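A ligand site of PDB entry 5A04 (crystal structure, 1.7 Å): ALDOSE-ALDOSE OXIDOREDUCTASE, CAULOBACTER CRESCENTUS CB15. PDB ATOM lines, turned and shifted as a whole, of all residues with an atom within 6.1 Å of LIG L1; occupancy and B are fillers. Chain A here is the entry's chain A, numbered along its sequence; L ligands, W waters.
N of Thr 265 is in hydrogen-bond range of OD1 of Asn 248, at 2.7 Å.
The side-chain hydroxyl of Tyr 189 is in hydrogen-bond range of the guanidinium group of Arg 132 (3.5 Å).
The guanidinium group of Arg 132 sits at hydrogen-bond distance from the backbone carbonyl oxygen of Ser 266, 3.3 Å away.
O of Thr 265 is in hydrogen-bond range of NH1 of Arg 132, 2.8 Å away.
The side-chain carboxylate of Asp 185 lies within salt-bridge range of the side-chain amino group of Lys 104 (3.9 Å).
The side-chain carboxylate (OD1) of Asp 185 is in salt-bridge range of the guanidinium group (NE) of Arg 172 (2.8 Å).
Phe 163 touches LIG L1.
Thr 265 touches LIG L1 (O to O6, 3.8 Å).
Tyr 267 touches LIG L1.
Hydrophobic or aromatic side chains within 4 Å of LIG L1: Phe 163 and Tyr 189.
Within 4 Å of LIG L1: Lys 104, Arg 132, Phe 163, Arg 172, Asp 185, Tyr 189, Thr 265 and Tyr 267.
The nearest printed residue that does not touch LIG L1 is Ile 186 (4.2 Å).
A nitrogen (N7) of LG2 L2 lies within hydrogen-bond range of the side-chain carboxylate (OE1) of Glu 103 (2.9 Å).
O9 of LG2 L2 lies within salt-bridge range of NH2 of Arg 172, at 2.8 Å.
The side-chain hydroxyl of Tyr 189 is in hydrogen-bond range of an oxygen (O1) of LIG L1, at 2.4 Å.
NZ of Lys 104 lies within hydrogen-bond range of O1 of LIG L1 (2.6 Å).
An oxygen (O6) of LIG L1 lies within hydrogen-bond range of the guanidinium group (NH2) of Arg 132 (3.3 Å).
The backbone carbonyl oxygen (O) of Lys 104 sits at hydrogen-bond distance from an oxygen (O13) of LG2 L2 (2.8 Å).
An oxygen (O2) of LIG L1 lies within hydrogen-bond range of the guanidinium group (NH2) of Arg 172, 3.2 Å away.
An oxygen (O13) of LG2 L2 lies within hydrogen-bond range of the side-chain amino group of Lys 104 (3.2 Å).
O14 of LG2 L2 lies within hydrogen-bond range of OH of Tyr 189 (3.1 Å).
An oxygen (O14) of LG2 L2 sits at hydrogen-bond distance from the guanidinium group (NE) of Arg 132.
The side-chain carboxylate (OD1) of Asp 185 sits at hydrogen-bond distance from an oxygen (O2) of LIG L1, 2.7 Å away.
Water W4 lies within hydrogen-bond range of O4 of LIG L1 and OH of Tyr 267.
Water W1 lies within hydrogen-bond range of OG1 of Thr 265 (2.8 Å), O6 of LIG L1 (3.0 Å) and ND2 of Asn 248 (3.3 Å).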
ATOM      1  N   GLU A 103      25.380  19.363 -16.940  1.00  0.00           N
ATOM      2  CA  GLU A 103      26.194  19.456 -18.151  1.00  0.00           C
ATOM      3  C   GLU A 103      27.159  20.641 -18.101  1.00  0.00           C
ATOM      4  O   GLU A 103      26.962  21.572 -17.335  1.00  0.00           O
ATOM      5  CB  GLU A 103      25.302  19.562 -19.397  1.00  0.00           C
ATOM      6  CG  GLU A 103      25.189  18.228 -20.129  1.00  0.00           C
ATOM      7  CD  GLU A 103      26.546  17.579 -20.311  1.00  0.00           C
ATOM      8  OE1 GLU A 103      27.457  18.268 -20.812  1.00  0.00           O
ATOM      9  OE2 GLU A 103      26.710  16.400 -19.930  1.00  0.00           O
ATOM     10  N   LYS A 104      28.219  20.571 -18.900  1.00  0.00           N
ATOM     11  CA  LYS A 104      29.104  21.705 -19.109  1.00  0.00           C
ATOM     12  C   LYS A 104      28.465  22.684 -20.089  1.00  0.00           C
ATOM     13  O   LYS A 104      27.560  22.326 -20.832  1.00  0.00           O
ATOM     14  CB  LYS A 104      30.473  21.251 -19.621  1.00  0.00           C
ATOM     15  CG  LYS A 104      30.484  20.102 -20.658  1.00  0.00           C
ATOM     16  CD  LYS A 104      29.737  20.401 -21.972  1.00  0.00           C
ATOM     17  CE  LYS A 104      30.294  21.604 -22.733  1.00  0.00           C
ATOM     18  NZ  LYS A 104      29.476  21.887 -23.950  1.00  0.00           N
ATOM     19  N   ARG A 132      32.624  14.122 -19.878  1.00  0.00           N
ATOM     20  CA  ARG A 132      32.668  12.718 -20.302  1.00  0.00           C
ATOM     21  C   ARG A 132      34.042  12.278 -20.797  1.00  0.00           C
ATOM     22  O   ARG A 132      34.357  11.084 -20.749  1.00  0.00           O
ATOM     23  CB  ARG A 132      31.618  12.479 -21.396  1.00  0.00           C
ATOM     24  CG  ARG A 132      31.691  13.458 -22.548  1.00  0.00           C
ATOM     25  CD  ARG A 132      30.788  13.059 -23.715  1.00  0.00           C
ATOM     26  NE  ARG A 132      30.775  14.129 -24.696  1.00  0.00           N
ATOM     27  CZ  ARG A 132      31.701  14.312 -25.629  1.00  0.00           C
ATOM     28  NH1 ARG A 132      32.703  13.445 -25.768  1.00  0.00           N
ATOM     29  NH2 ARG A 132      31.601  15.351 -26.450  1.00  0.00           N
ATOM     30  N   PHE A 163      33.345  24.045 -34.028  1.00  0.00           N
ATOM     31  CA  PHE A 163      32.529  23.497 -35.113  1.00  0.00           C
ATOM     32  C   PHE A 163      31.841  24.652 -35.819  1.00  0.00           C
ATOM     33  O   PHE A 163      31.735  25.754 -35.280  1.00  0.00           O
ATOM     34  CB  PHE A 163      31.517  22.460 -34.610  1.00  0.00           C
ATOM     35  CG  PHE A 163      30.400  23.011 -33.758  1.00  0.00           C
ATOM     36  CD1 PHE A 163      30.583  23.214 -32.401  1.00  0.00           C
ATOM     37  CD2 PHE A 163      29.156  23.279 -34.318  1.00  0.00           C
ATOM     38  CE1 PHE A 163      29.542  23.706 -31.613  1.00  0.00           C
ATOM     39  CE2 PHE A 163      28.110  23.775 -33.538  1.00  0.00           C
ATOM     40  CZ  PHE A 163      28.307  23.986 -32.190  1.00  0.00           C
ATOM     41  N   ARG A 172      22.411  28.662 -28.300  1.00  0.00           N
ATOM     42  CA  ARG A 172      23.857  28.862 -28.168  1.00  0.00           C
ATOM     43  C   ARG A 172      24.344  30.236 -28.652  1.00  0.00           C
ATOM     44  O   ARG A 172      25.411  30.692 -28.259  1.00  0.00           O
ATOM     45  CB  ARG A 172      24.624  27.763 -28.918  1.00  0.00           C
ATOM     46  CG  ARG A 172      24.737  26.443 -28.148  1.00  0.00           C
ATOM     47  CD  ARG A 172      25.358  25.363 -29.028  1.00  0.00           C
ATOM     48  NE  ARG A 172      25.546  24.099 -28.299  1.00  0.00           N
ATOM     49  CZ  ARG A 172      24.595  23.192 -28.100  1.00  0.00           C
ATOM     50  NH1 ARG A 172      23.361  23.385 -28.562  1.00  0.00           N
ATOM     51  NH2 ARG A 172      24.875  22.061 -27.447  1.00  0.00           N
ATOM     52  N   ASP A 185      30.836  26.847 -25.068  1.00  0.00           N
ATOM     53  CA  ASP A 185      30.274  25.613 -25.602  1.00  0.00           C
ATOM     54  C   ASP A 185      31.277  24.547 -25.984  1.00  0.00           C
ATOM     55  O   ASP A 185      31.088  23.364 -25.674  1.00  0.00           O
ATOM     56  CB  ASP A 185      29.422  25.914 -26.839  1.00  0.00           C
ATOM     57  CG  ASP A 185      28.723  24.681 -27.366  1.00  0.00           C
ATOM     58  OD1 ASP A 185      27.798  24.188 -26.682  1.00  0.00           O
ATOM     59  OD2 ASP A 185      29.120  24.190 -28.446  1.00  0.00           O
ATOM     60  N   ILE A 186      32.313  24.949 -26.706  1.00  0.00           N
ATOM     61  CA  ILE A 186      33.204  23.987 -27.321  1.00  0.00           C
ATOM     62  C   ILE A 186      34.652  24.279 -26.941  1.00  0.00           C
ATOM     63  O   ILE A 186      35.461  23.370 -26.735  1.00  0.00           O
ATOM     64  CB  ILE A 186      32.972  23.966 -28.876  1.00  0.00           C
ATOM     65  CG1 ILE A 186      33.894  22.954 -29.540  1.00  0.00           C
ATOM     66  CG2 ILE A 186      33.106  25.349 -29.496  1.00  0.00           C
ATOM     67  CD1 ILE A 186      33.651  21.547 -29.045  1.00  0.00           C
ATOM     68  N   ILE A 188      35.628  25.274 -24.175  1.00  0.00           N
ATOM     69  CA  ILE A 188      35.825  24.715 -22.848  1.00  0.00           C
ATOM     70  C   ILE A 188      36.514  23.335 -22.899  1.00  0.00           C
ATOM     71  O   ILE A 188      37.219  22.961 -21.960  1.00  0.00           O
ATOM     72  CB  ILE A 188      34.471  24.636 -22.097  1.00  0.00           C
ATOM     73  CG1 ILE A 188      34.680  24.282 -20.619  1.00  0.00           C
ATOM     74  CG2 ILE A 188      33.538  23.661 -22.809  1.00  0.00           C
ATOM     75  CD1 ILE A 188      33.434  24.533 -19.774  1.00  0.00           C
ATOM     76  N   TYR A 189      36.336  22.582 -23.988  1.00  0.00           N
ATOM     77  CA  TYR A 189      37.063  21.301 -24.085  1.00  0.00           C
ATOM     78  C   TYR A 189      38.575  21.509 -24.203  1.00  0.00           C
ATOM     79  O   TYR A 189      39.364  20.696 -23.698  1.00  0.00           O
ATOM     80  CB  TYR A 189      36.576  20.462 -25.277  1.00  0.00           C
ATOM     81  CG  TYR A 189      35.197  19.880 -25.077  1.00  0.00           C
ATOM     82  CD1 TYR A 189      34.065  20.582 -25.459  1.00  0.00           C
ATOM     83  CD2 TYR A 189      35.039  18.613 -24.525  1.00  0.00           C
ATOM     84  CE1 TYR A 189      32.796  20.045 -25.293  1.00  0.00           C
ATOM     85  CE2 TYR A 189      33.778  18.064 -24.357  1.00  0.00           C
ATOM     86  CZ  TYR A 189      32.660  18.781 -24.744  1.00  0.00           C
ATOM     87  OH  TYR A 189      31.412  18.241 -24.569  1.00  0.00           O
ATOM     88  N   TYR A 243      33.601  28.962 -33.591  1.00  0.00           N
ATOM     89  CA  TYR A 243      32.281  28.614 -34.093  1.00  0.00           C
ATOM     90  C   TYR A 243      32.221  28.695 -35.625  1.00  0.00           C
ATOM     91  O   TYR A 243      31.154  28.604 -36.220  1.00  0.00           O
ATOM     92  CB  TYR A 243      31.221  29.563 -33.490  1.00  0.00           C
ATOM     93  CG  TYR A 243      30.460  29.048 -32.274  1.00  0.00           C
ATOM     94  CD1 TYR A 243      30.424  27.711 -31.943  1.00  0.00           C
ATOM     95  CD2 TYR A 243      29.751  29.941 -31.471  1.00  0.00           C
ATOM     96  CE1 TYR A 243      29.699  27.255 -30.845  1.00  0.00           C
ATOM     97  CE2 TYR A 243      29.026  29.509 -30.376  1.00  0.00           C
ATOM     98  CZ  TYR A 243      28.993  28.170 -30.061  1.00  0.00           C
ATOM     99  OH  TYR A 243      28.253  27.762 -28.970  1.00  0.00           O
ATOM    100  N   ASN A 248      38.941  19.331 -33.552  1.00  0.00           N
ATOM    101  CA  ASN A 248      38.741  18.630 -32.307  1.00  0.00           C
ATOM    102  C   ASN A 248      39.954  17.786 -32.045  1.00  0.00           C
ATOM    103  O   ASN A 248      40.040  16.655 -32.538  1.00  0.00           O
ATOM    104  CB  ASN A 248      37.476  17.750 -32.352  1.00  0.00           C
ATOM    105  CG  ASN A 248      37.108  17.197 -30.978  1.00  0.00           C
ATOM    106  OD1 ASN A 248      37.941  16.605 -30.301  1.00  0.00           O
ATOM    107  ND2 ASN A 248      35.882  17.428 -30.550  1.00  0.00           N
ATOM    108  N   THR A 265      37.731  14.590 -28.471  1.00  0.00           N
ATOM    109  CA  THR A 265      36.649  14.636 -27.467  1.00  0.00           C
ATOM    110  C   THR A 265      35.288  14.491 -28.137  1.00  0.00           C
ATOM    111  O   THR A 265      34.250  14.936 -27.638  1.00  0.00           O
ATOM    112  CB  THR A 265      36.708  15.952 -26.654  1.00  0.00           C
ATOM    113  OG1 THR A 265      36.536  17.052 -27.540  1.00  0.00           O
ATOM    114  CG2 THR A 265      38.055  16.081 -25.938  1.00  0.00           C
ATOM    115  N   SER A 266      35.295  13.830 -29.290  1.00  0.00           N
ATOM    116  CA  SER A 266      34.079  13.543 -30.023  1.00  0.00           C
ATOM    117  C   SER A 266      33.291  12.414 -29.364  1.00  0.00           C
ATOM    118  O   SER A 266      33.780  11.779 -28.437  1.00  0.00           O
ATOM    119  CB  SER A 266      34.430  13.173 -31.457  1.00  0.00           C
ATOM    120  OG  SER A 266      35.437  12.178 -31.446  1.00  0.00           O
ATOM    121  N   TYR A 267      32.061  12.172 -29.828  1.00  0.00           N
ATOM    122  CA  TYR A 267      31.240  11.107 -29.251  1.00  0.00           C
ATOM    123  C   TYR A 267      31.841   9.729 -29.534  1.00  0.00           C
ATOM    124  O   TYR A 267      31.751   8.808 -28.719  1.00  0.00           O
ATOM    125  CB  TYR A 267      29.802  11.175 -29.802  1.00  0.00           C
ATOM    126  CG  TYR A 267      29.057  12.477 -29.540  1.00  0.00           C
ATOM    127  CD1 TYR A 267      29.335  13.257 -28.415  1.00  0.00           C
ATOM    128  CD2 TYR A 267      28.051  12.908 -30.403  1.00  0.00           C
ATOM    129  CE1 TYR A 267      28.640  14.436 -28.168  1.00  0.00           C
ATOM    130  CE2 TYR A 267      27.358  14.094 -30.168  1.00  0.00           C
ATOM    131  CZ  TYR A 267      27.659  14.846 -29.048  1.00  0.00           C
ATOM    132  OH  TYR A 267      26.972  16.028 -28.805  1.00  0.00           O
HETATM  133  C1  LIG L   1      28.833  20.910 -27.319  1.00  0.00           C
HETATM  134  C2  LIG L   1      28.230  20.627 -28.709  1.00  0.00           C
HETATM  135  C3  LIG L   1      29.249  19.967 -29.595  1.00  0.00           C
HETATM  136  C4  LIG L   1      29.864  18.762 -28.918  1.00  0.00           C
HETATM  137  C5  LIG L   1      31.064  18.255 -29.767  1.00  0.00           C
HETATM  138  C6  LIG L   1      29.314  19.629 -26.825  1.00  0.00           C
HETATM  139  O1  LIG L   1      29.766  19.768 -25.478  1.00  0.00           O
HETATM  140  O2  LIG L   1      27.827  21.465 -26.491  1.00  0.00           O
HETATM  141  O3  LIG L   1      27.814  21.872 -29.248  1.00  0.00           O
HETATM  142  O4  LIG L   1      28.631  19.575 -30.812  1.00  0.00           O
HETATM  143  O5  LIG L   1      30.360  19.093 -27.637  1.00  0.00           O
HETATM  144  O6  LIG L   1      31.543  17.000 -29.259  1.00  0.00           O
HETATM  145  P1  LG2 L   2      19.037  21.436 -27.136  1.00  0.00           P
HETATM  146  O1  LG2 L   2      18.624  22.803 -27.539  1.00  0.00           O
HETATM  147  O2  LG2 L   2      19.140  20.365 -28.190  1.00  0.00           O
HETATM  148  O3  LG2 L   2      18.074  20.861 -25.939  1.00  0.00           O
HETATM  149  C1  LG2 L   2      17.949  21.838 -24.949  1.00  0.00           C
HETATM  150  C2  LG2 L   2      16.701  21.447 -24.149  1.00  0.00           C
HETATM  151  O4  LG2 L   2      16.623  22.172 -22.921  1.00  0.00           O
HETATM  152  C3  LG2 L   2      15.434  21.795 -24.961  1.00  0.00           C
HETATM  153  O5  LG2 L   2      15.086  20.776 -25.838  1.00  0.00           O
HETATM  154  C4  LG2 L   2      14.385  21.841 -23.847  1.00  0.00           C
HETATM  155  O6  LG2 L   2      13.987  20.658 -23.482  1.00  0.00           O
HETATM  156  C5  LG2 L   2      15.254  22.396 -22.638  1.00  0.00           C
HETATM  157  N1  LG2 L   2      15.019  23.819 -22.374  1.00  0.00           N
HETATM  158  C6  LG2 L   2      14.534  24.375 -21.202  1.00  0.00           C
HETATM  159  N2  LG2 L   2      14.394  25.715 -21.268  1.00  0.00           N
HETATM  160  C7  LG2 L   2      14.818  26.039 -22.569  1.00  0.00           C
HETATM  161  C8  LG2 L   2      14.911  27.267 -23.250  1.00  0.00           C
HETATM  162  N3  LG2 L   2      14.559  28.438 -22.621  1.00  0.00           N
HETATM  163  N4  LG2 L   2      15.365  27.334 -24.538  1.00  0.00           N
HETATM  164  C9  LG2 L   2      15.708  26.112 -25.099  1.00  0.00           C
HETATM  165  N5  LG2 L   2      15.668  24.877 -24.579  1.00  0.00           N
HETATM  166  C10 LG2 L   2      15.210  24.861 -23.280  1.00  0.00           C
HETATM  167  O7  LG2 L   2      20.529  21.742 -26.480  1.00  0.00           O
HETATM  168  P2  LG2 L   2      21.557  20.489 -26.351  1.00  0.00           P
HETATM  169  O8  LG2 L   2      20.940  19.292 -25.759  1.00  0.00           O
HETATM  170  O9  LG2 L   2      22.585  20.454 -27.470  1.00  0.00           O
HETATM  171  O10 LG2 L   2      22.578  21.117 -25.073  1.00  0.00           O
HETATM  172  C11 LG2 L   2      21.924  21.203 -23.838  1.00  0.00           C
HETATM  173  C12 LG2 L   2      23.035  21.210 -22.746  1.00  0.00           C
HETATM  174  O11 LG2 L   2      23.878  20.041 -22.936  1.00  0.00           O
HETATM  175  C13 LG2 L   2      23.998  22.456 -22.890  1.00  0.00           C
HETATM  176  O12 LG2 L   2      24.437  22.882 -21.587  1.00  0.00           O
HETATM  177  C14 LG2 L   2      25.175  21.891 -23.661  1.00  0.00           C
HETATM  178  O13 LG2 L   2      26.393  22.538 -23.329  1.00  0.00           O
HETATM  179  C15 LG2 L   2      25.223  20.434 -23.093  1.00  0.00           C
HETATM  180  N6  LG2 L   2      25.797  19.513 -24.084  1.00  0.00           N
HETATM  181  C16 LG2 L   2      26.852  18.691 -23.731  1.00  0.00           C
HETATM  182  C17 LG2 L   2      27.357  17.817 -24.656  1.00  0.00           C
HETATM  183  C18 LG2 L   2      28.475  16.946 -24.283  1.00  0.00           C
HETATM  184  O14 LG2 L   2      29.082  16.260 -25.129  1.00  0.00           O
HETATM  185  N7  LG2 L   2      28.859  16.865 -22.947  1.00  0.00           N
HETATM  186  C19 LG2 L   2      26.830  17.734 -26.038  1.00  0.00           C
HETATM  187  C20 LG2 L   2      25.746  18.683 -26.337  1.00  0.00           C
HETATM  188  C21 LG2 L   2      25.270  19.503 -25.391  1.00  0.00           C
HETATM  189  P3  LG2 L   2      12.306  20.442 -23.137  1.00  0.00           P
HETATM  190  O15 LG2 L   2      12.086  21.542 -22.121  1.00  0.00           O
HETATM  191  O16 LG2 L   2      11.742  20.667 -24.503  1.00  0.00           O
HETATM  192  O17 LG2 L   2      12.272  19.003 -22.600  1.00  0.00           O
HETATM  193  O   HOH W   1      33.974  18.110 -27.890  1.00  0.00           O
HETATM  194  O   HOH W   2      33.625  18.273 -32.112  1.00  0.00           O
HETATM  195  O   HOH W   3      29.628  19.150 -32.957  1.00  0.00           O
HETATM  196  O   HOH W   4      26.355  17.959 -30.919  1.00  0.00           O
HETATM  197  O   HOH W   5      25.678  21.695 -30.991  1.00  0.00           O
